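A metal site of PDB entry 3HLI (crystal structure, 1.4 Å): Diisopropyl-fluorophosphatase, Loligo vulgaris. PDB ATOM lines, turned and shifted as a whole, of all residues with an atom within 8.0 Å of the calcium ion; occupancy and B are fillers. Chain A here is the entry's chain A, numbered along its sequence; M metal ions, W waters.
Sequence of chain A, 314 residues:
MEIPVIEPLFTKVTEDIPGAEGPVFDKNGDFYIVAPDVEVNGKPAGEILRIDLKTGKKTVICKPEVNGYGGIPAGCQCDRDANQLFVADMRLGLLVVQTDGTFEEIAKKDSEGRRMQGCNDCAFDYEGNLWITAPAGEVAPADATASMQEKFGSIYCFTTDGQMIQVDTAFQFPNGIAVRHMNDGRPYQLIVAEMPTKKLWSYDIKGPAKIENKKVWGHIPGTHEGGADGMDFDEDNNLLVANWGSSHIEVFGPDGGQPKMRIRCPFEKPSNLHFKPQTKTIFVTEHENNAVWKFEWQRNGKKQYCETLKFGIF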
ATOM      1  N   GLU A  21      34.740  -6.436   1.175  1.00  0.00           N
ATOM      2  CA  GLU A  21      33.460  -7.061   0.884  1.00  0.00           C
ATOM      3  C   GLU A  21      33.103  -8.142   1.893  1.00  0.00           C
ATOM      4  O   GLU A  21      33.817  -8.343   2.882  1.00  0.00           O
ATOM      5  CB  GLU A  21      33.494  -7.678  -0.523  1.00  0.00           C
ATOM      6  CG  GLU A  21      32.690  -6.925  -1.574  1.00  0.00           C
ATOM      7  CD  GLU A  21      31.220  -7.294  -1.545  1.00  0.00           C
ATOM      8  OE1 GLU A  21      30.767  -7.908  -0.553  1.00  0.00           O
ATOM      9  OE2 GLU A  21      30.518  -6.973  -2.531  1.00  0.00           O
ATOM     10  N   GLY A  22      32.007  -8.823   1.623  1.00  0.00           N
ATOM     11  CA  GLY A  22      31.537  -9.935   2.442  1.00  0.00           C
ATOM     12  C   GLY A  22      31.565  -9.840   3.946  1.00  0.00           C
ATOM     13  O   GLY A  22      32.067 -10.761   4.607  1.00  0.00           O
ATOM     14  N   PRO A  23      31.038  -8.764   4.552  1.00  0.00           N
ATOM     15  CA  PRO A  23      31.049  -8.663   6.004  1.00  0.00           C
ATOM     16  C   PRO A  23      30.140  -9.743   6.577  1.00  0.00           C
ATOM     17  O   PRO A  23      29.055 -10.001   6.045  1.00  0.00           O
ATOM     18  CB  PRO A  23      30.521  -7.257   6.258  1.00  0.00           C
ATOM     19  CG  PRO A  23      29.585  -7.035   5.100  1.00  0.00           C
ATOM     20  CD  PRO A  23      30.364  -7.604   3.933  1.00  0.00           C
ATOM     21  N   VAL A  24      30.589 -10.399   7.640  1.00  0.00           N
ATOM     22  CA  VAL A  24      29.802 -11.464   8.234  1.00  0.00           C
ATOM     23  C   VAL A  24      30.218 -11.718   9.679  1.00  0.00           C
ATOM     24  O   VAL A  24      31.371 -11.498  10.049  1.00  0.00           O
ATOM     25  CB  VAL A  24      29.940 -12.775   7.402  1.00  0.00           C
ATOM     26  CG1 VAL A  24      31.365 -13.303   7.494  1.00  0.00           C
ATOM     27  CG2 VAL A  24      28.945 -13.824   7.889  1.00  0.00           C
ATOM     28  N   PHE A  25      29.266 -12.181  10.490  1.00  0.00           N
ATOM     29  CA  PHE A  25      29.523 -12.533  11.879  1.00  0.00           C
ATOM     30  C   PHE A  25      29.336 -14.039  11.999  1.00  0.00           C
ATOM     31  O   PHE A  25      28.421 -14.593  11.397  1.00  0.00           O
ATOM     32  CB  PHE A  25      28.529 -11.826  12.812  1.00  0.00           C
ATOM     33  CG  PHE A  25      28.883 -10.395  13.099  1.00  0.00           C
ATOM     34  CD1 PHE A  25      29.815 -10.087  14.081  1.00  0.00           C
ATOM     35  CD2 PHE A  25      28.276  -9.359  12.398  1.00  0.00           C
ATOM     36  CE1 PHE A  25      30.155  -8.763  14.361  1.00  0.00           C
ATOM     37  CE2 PHE A  25      28.603  -8.030  12.660  1.00  0.00           C
ATOM     38  CZ  PHE A  25      29.551  -7.730  13.650  1.00  0.00           C
ATOM     39  N   CYS A  76      30.086 -13.725   1.860  1.00  0.00           N
ATOM     40  CA  CYS A  76      30.017 -14.771   2.881  1.00  0.00           C
ATOM     41  C   CYS A  76      28.683 -14.925   3.587  1.00  0.00           C
ATOM     42  O   CYS A  76      27.874 -13.994   3.671  1.00  0.00           O
ATOM     43  CB  CYS A  76      31.042 -14.505   3.998  1.00  0.00           C
ATOM     44  SG  CYS A  76      32.698 -14.024   3.498  1.00  0.00           S
ATOM     45  N   GLN A  77      28.497 -16.124   4.141  1.00  0.00           N
ATOM     46  CA  GLN A  77      27.338 -16.482   4.953  1.00  0.00           C
ATOM     47  C   GLN A  77      27.869 -17.474   5.978  1.00  0.00           C
ATOM     48  O   GLN A  77      28.731 -18.303   5.663  1.00  0.00           O
ATOM     49  CB  GLN A  77      26.246 -17.171   4.132  1.00  0.00           C
ATOM     50  CG  GLN A  77      25.405 -16.271   3.246  1.00  0.00           C
ATOM     51  CD  GLN A  77      24.560 -15.292   4.024  1.00  0.00           C
ATOM     52  OE1 GLN A  77      25.025 -14.214   4.413  1.00  0.00           O
ATOM     53  NE2 GLN A  77      23.311 -15.652   4.279  1.00  0.00           N
ATOM     54  N   ASP A 121      28.187 -13.318  -4.255  1.00  0.00           N
ATOM     55  CA  ASP A 121      27.574 -13.243  -2.925  1.00  0.00           C
ATOM     56  C   ASP A 121      26.616 -14.406  -2.758  1.00  0.00           C
ATOM     57  O   ASP A 121      26.300 -15.115  -3.718  1.00  0.00           O
ATOM     58  CB  ASP A 121      26.831 -11.907  -2.756  1.00  0.00           C
ATOM     59  CG  ASP A 121      26.799 -11.425  -1.298  1.00  0.00           C
ATOM     60  OD1 ASP A 121      27.181 -12.192  -0.383  1.00  0.00           O
ATOM     61  OD2 ASP A 121      26.395 -10.262  -1.069  1.00  0.00           O
ATOM     62  N   CYS A 122      26.141 -14.612  -1.538  1.00  0.00           N
ATOM     63  CA  CYS A 122      25.211 -15.691  -1.272  1.00  0.00           C
ATOM     64  C   CYS A 122      24.332 -15.374  -0.071  1.00  0.00           C
ATOM     65  O   CYS A 122      24.659 -14.520   0.751  1.00  0.00           O
ATOM     66  CB  CYS A 122      25.967 -17.019  -1.062  1.00  0.00           C
ATOM     67  SG  CYS A 122      27.254 -17.014   0.222  1.00  0.00           S
ATOM     68  N   ILE A 177      22.126 -10.559  -3.130  1.00  0.00           N
ATOM     69  CA  ILE A 177      21.034 -11.533  -3.135  1.00  0.00           C
ATOM     70  C   ILE A 177      20.485 -11.649  -1.715  1.00  0.00           C
ATOM     71  O   ILE A 177      21.233 -11.514  -0.743  1.00  0.00           O
ATOM     72  CB  ILE A 177      21.553 -12.898  -3.683  1.00  0.00           C
ATOM     73  CG1 ILE A 177      20.399 -13.886  -3.886  1.00  0.00           C
ATOM     74  CG2 ILE A 177      22.607 -13.467  -2.756  1.00  0.00           C
ATOM     75  CD1 ILE A 177      20.739 -15.043  -4.829  1.00  0.00           C
ATOM     76  N   GLY A 230      25.691  -5.379  -2.369  1.00  0.00           N
ATOM     77  CA  GLY A 230      25.153  -6.229  -1.308  1.00  0.00           C
ATOM     78  C   GLY A 230      23.839  -5.779  -0.680  1.00  0.00           C
ATOM     79  O   GLY A 230      23.481  -4.606  -0.736  1.00  0.00           O
ATOM     80  N   MET A 231      23.129  -6.726  -0.068  1.00  0.00           N
ATOM     81  CA  MET A 231      21.846  -6.431   0.561  1.00  0.00           C
ATOM     82  C   MET A 231      21.530  -7.327   1.743  1.00  0.00           C
ATOM     83  O   MET A 231      22.111  -8.399   1.901  1.00  0.00           O
ATOM     84  CB  MET A 231      20.723  -6.601  -0.467  1.00  0.00           C
ATOM     85  CG  MET A 231      20.650  -8.004  -1.043  1.00  0.00           C
ATOM     86  SD  MET A 231      19.297  -8.204  -2.206  1.00  0.00           S
ATOM     87  CE  MET A 231      19.543  -6.717  -3.220  1.00  0.00           C
ATOM     88  N   ASP A 232      20.603  -6.871   2.586  1.00  0.00           N
ATOM     89  CA  ASP A 232      20.149  -7.622   3.750  1.00  0.00           C
ATOM     90  C   ASP A 232      18.838  -7.024   4.236  1.00  0.00           C
ATOM     91  O   ASP A 232      18.578  -5.836   4.036  1.00  0.00           O
ATOM     92  CB  ASP A 232      21.147  -7.569   4.897  1.00  0.00           C
ATOM     93  CG  ASP A 232      22.093  -8.753   4.917  1.00  0.00           C
ATOM     94  OD1 ASP A 232      21.683  -9.890   4.600  1.00  0.00           O
ATOM     95  OD2 ASP A 232      23.270  -8.535   5.286  1.00  0.00           O
ATOM     96  N   PHE A 233      18.035  -7.846   4.887  1.00  0.00           N
ATOM     97  CA  PHE A 233      16.748  -7.417   5.443  1.00  0.00           C
ATOM     98  C   PHE A 233      16.899  -6.992   6.899  1.00  0.00           C
ATOM     99  O   PHE A 233      17.756  -7.512   7.614  1.00  0.00           O
ATOM    100  CB  PHE A 233      15.750  -8.571   5.415  1.00  0.00           C
ATOM    101  CG  PHE A 233      15.143  -8.824   4.066  1.00  0.00           C
ATOM    102  CD1 PHE A 233      14.209  -7.948   3.540  1.00  0.00           C
ATOM    103  CD2 PHE A 233      15.483  -9.964   3.351  1.00  0.00           C
ATOM    104  CE1 PHE A 233      13.620  -8.192   2.306  1.00  0.00           C
ATOM    105  CE2 PHE A 233      14.893 -10.219   2.109  1.00  0.00           C
ATOM    106  CZ  PHE A 233      13.963  -9.334   1.582  1.00  0.00           C
ATOM    107  N   LEU A 240      17.687  -3.441   2.786  1.00  0.00           N
ATOM    108  CA  LEU A 240      18.721  -2.419   2.689  1.00  0.00           C
ATOM    109  C   LEU A 240      19.692  -2.871   1.607  1.00  0.00           C
ATOM    110  O   LEU A 240      20.204  -3.995   1.631  1.00  0.00           O
ATOM    111  CB  LEU A 240      19.432  -2.236   4.032  1.00  0.00           C
ATOM    112  CG  LEU A 240      18.599  -1.540   5.118  1.00  0.00           C
ATOM    113  CD1 LEU A 240      17.612  -2.515   5.731  1.00  0.00           C
ATOM    114  CD2 LEU A 240      19.521  -0.990   6.192  1.00  0.00           C
ATOM    115  N   ASN A 272      28.846  -3.616   0.514  1.00  0.00           N
ATOM    116  CA  ASN A 272      28.021  -4.597   1.191  1.00  0.00           C
ATOM    117  C   ASN A 272      27.757  -4.171   2.631  1.00  0.00           C
ATOM    118  O   ASN A 272      28.302  -3.166   3.104  1.00  0.00           O
ATOM    119  CB  ASN A 272      28.714  -5.965   1.155  1.00  0.00           C
ATOM    120  CG  ASN A 272      27.731  -7.104   0.973  1.00  0.00           C
ATOM    121  OD1 ASN A 272      26.605  -7.045   1.476  1.00  0.00           O
ATOM    122  ND2 ASN A 272      28.147  -8.136   0.267  1.00  0.00           N
ATOM    123  N   LEU A 273      26.929  -4.930   3.320  1.00  0.00           N
ATOM    124  CA  LEU A 273      26.590  -4.616   4.697  1.00  0.00           C
ATOM    125  C   LEU A 273      26.171  -5.865   5.453  1.00  0.00           C
ATOM    126  O   LEU A 273      25.881  -6.906   4.866  1.00  0.00           O
ATOM    127  CB  LEU A 273      25.460  -3.579   4.715  1.00  0.00           C
ATOM    128  CG  LEU A 273      24.180  -3.873   3.929  1.00  0.00           C
ATOM    129  CD1 LEU A 273      23.316  -4.861   4.671  1.00  0.00           C
ATOM    130  CD2 LEU A 273      23.409  -2.571   3.720  1.00  0.00           C
ATOM    131  N   HIS A 274      26.160  -5.760   6.784  1.00  0.00           N
ATOM    132  CA  HIS A 274      25.756  -6.874   7.618  1.00  0.00           C
ATOM    133  C   HIS A 274      25.433  -6.360   9.020  1.00  0.00           C
ATOM    134  O   HIS A 274      26.150  -5.506   9.538  1.00  0.00           O
ATOM    135  CB  HIS A 274      26.883  -7.902   7.707  1.00  0.00           C
ATOM    136  CG  HIS A 274      26.400  -9.306   7.895  1.00  0.00           C
ATOM    137  ND1 HIS A 274      25.798 -10.020   6.881  1.00  0.00           N
ATOM    138  CD2 HIS A 274      26.455 -10.143   8.958  1.00  0.00           C
ATOM    139  CE1 HIS A 274      25.507 -11.238   7.311  1.00  0.00           C
ATOM    140  NE2 HIS A 274      25.892 -11.338   8.566  1.00  0.00           N
ATOM    141  N   PHE A 275      24.354  -6.849   9.601  1.00  0.00           N
ATOM    142  CA  PHE A 275      23.969  -6.442  10.945  1.00  0.00           C
ATOM    143  C   PHE A 275      24.746  -7.226  11.994  1.00  0.00           C
ATOM    144  O   PHE A 275      25.097  -8.381  11.776  1.00  0.00           O
ATOM    145  CB  PHE A 275      22.479  -6.712  11.225  1.00  0.00           C
ATOM    146  CG  PHE A 275      21.542  -5.727  10.600  1.00  0.00           C
ATOM    147  CD1 PHE A 275      21.173  -5.849   9.261  1.00  0.00           C
ATOM    148  CD2 PHE A 275      20.975  -4.710  11.363  1.00  0.00           C
ATOM    149  CE1 PHE A 275      20.266  -4.969   8.688  1.00  0.00           C
ATOM    150  CE2 PHE A 275      20.061  -3.824  10.809  1.00  0.00           C
ATOM    151  CZ  PHE A 275      19.704  -3.953   9.465  1.00  0.00           C
ATOM    152  N   ILE A 282      24.888  -1.695  11.887  1.00  0.00           N
ATOM    153  CA  ILE A 282      25.160  -2.211  10.554  1.00  0.00           C
ATOM    154  C   ILE A 282      26.600  -1.909  10.167  1.00  0.00           C
ATOM    155  O   ILE A 282      27.049  -0.766  10.231  1.00  0.00           O
ATOM    156  CB  ILE A 282      24.243  -1.567   9.492  1.00  0.00           C
ATOM    157  CG1 ILE A 282      22.780  -1.898   9.778  1.00  0.00           C
ATOM    158  CG2 ILE A 282      24.638  -2.053   8.097  1.00  0.00           C
ATOM    159  CD1 ILE A 282      21.804  -1.323   8.757  1.00  0.00           C
ATOM    160  N   PHE A 283      27.324  -2.952   9.783  1.00  0.00           N
ATOM    161  CA  PHE A 283      28.698  -2.791   9.334  1.00  0.00           C
ATOM    162  C   PHE A 283      28.655  -2.683   7.820  1.00  0.00           C
ATOM    163  O   PHE A 283      27.960  -3.457   7.155  1.00  0.00           O
ATOM    164  CB  PHE A 283      29.558  -3.962   9.806  1.00  0.00           C
ATOM    165  CG  PHE A 283      29.893  -3.905  11.262  1.00  0.00           C
ATOM    166  CD1 PHE A 283      28.935  -4.192  12.231  1.00  0.00           C
ATOM    167  CD2 PHE A 283      31.156  -3.490  11.685  1.00  0.00           C
ATOM    168  CE1 PHE A 283      29.219  -4.067  13.592  1.00  0.00           C
ATOM    169  CE2 PHE A 283      31.455  -3.363  13.040  1.00  0.00           C
ATOM    170  CZ  PHE A 283      30.480  -3.654  13.992  1.00  0.00           C
ATOM    171  N   GLN A 304      20.001 -13.996  10.606  1.00  0.00           N
ATOM    172  CA  GLN A 304      20.637 -14.752   9.549  1.00  0.00           C
ATOM    173  C   GLN A 304      20.382 -16.214   9.908  1.00  0.00           C
ATOM    174  O   GLN A 304      20.045 -16.527  11.046  1.00  0.00           O
ATOM    175  CB  GLN A 304      22.142 -14.484   9.519  1.00  0.00           C
ATOM    176  CG  GLN A 304      22.532 -13.123   8.975  1.00  0.00           C
ATOM    177  CD  GLN A 304      22.519 -13.090   7.450  1.00  0.00           C
ATOM    178  OE1 GLN A 304      21.630 -12.511   6.828  1.00  0.00           O
ATOM    179  NE2 GLN A 304      23.514 -13.716   6.850  1.00  0.00           N
HETATM  180 CA    CA M   1      25.299  -9.126   4.608  1.00  0.00          CA
HETATM  181  O   HOH W   1      27.476  -9.602   3.954  1.00  0.00           O
HETATM  182  O   HOH W   2      24.176 -11.181   4.193  1.00  0.00           O
HETATM  183  O   HOH W   3      24.809  -8.739   2.385  1.00  0.00           O
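The side-chain carboxylate (OD1) of Asp 232 lies close to the side-chain amide oxygen (OE1) of Gln 304 (3.4 Å).
The side-chain amide nitrogen of Asn 272 sits at hydrogen-bond distance from the side-chain carboxylate of Asp 121 (3.1 Å).
The backbone carbonyl oxygen of His 274 is in hydrogen-bond range of the backbone NH of Phe 283 (2.8 Å).
The side-chain amide nitrogen (ND2) of Asn 272 lies within hydrogen-bond range of the side-chain carboxylate (OE1) of Glu 21 (2.8 Å).
N of Leu 240 sits at hydrogen-bond distance from O of Asp 232 (2.8 Å).
O of Pro 23 sits close to ND1 of His 274 (3.4 Å).
Residues that only touch the calcium ion: Asn 272.
Within 4 Å of the calcium ion: Asp 232, Asn 272, Leu 273 and His 274.
The nearest printed residue that does not touch the calcium ion is Pro 23 (4.1 Å).
The calcium ion is bound by OD2 of Asp 232.
The calcium ion is bound by water W3 (2.3 Å).
The calcium ion is bound by the backbone carbonyl oxygen (O) of Leu 273 (2.3 Å).
The calcium ion is bound by water W1, at 2.3 Å.
The calcium ion is bound by water W2, 2.4 Å away.
ND1 of His 274 binds the calcium ion, at 2.5 Å.
Water W3 bridges the side-chain amide oxygen of Asn 272 (2.6 Å) and the backbone carbonyl oxygen of Met 231 (2.8 Å).
Water W2 lies within hydrogen-bond range of OD1 of Asp 232 (2.8 Å) and OE1 of Gln 77 (3.2 Å).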
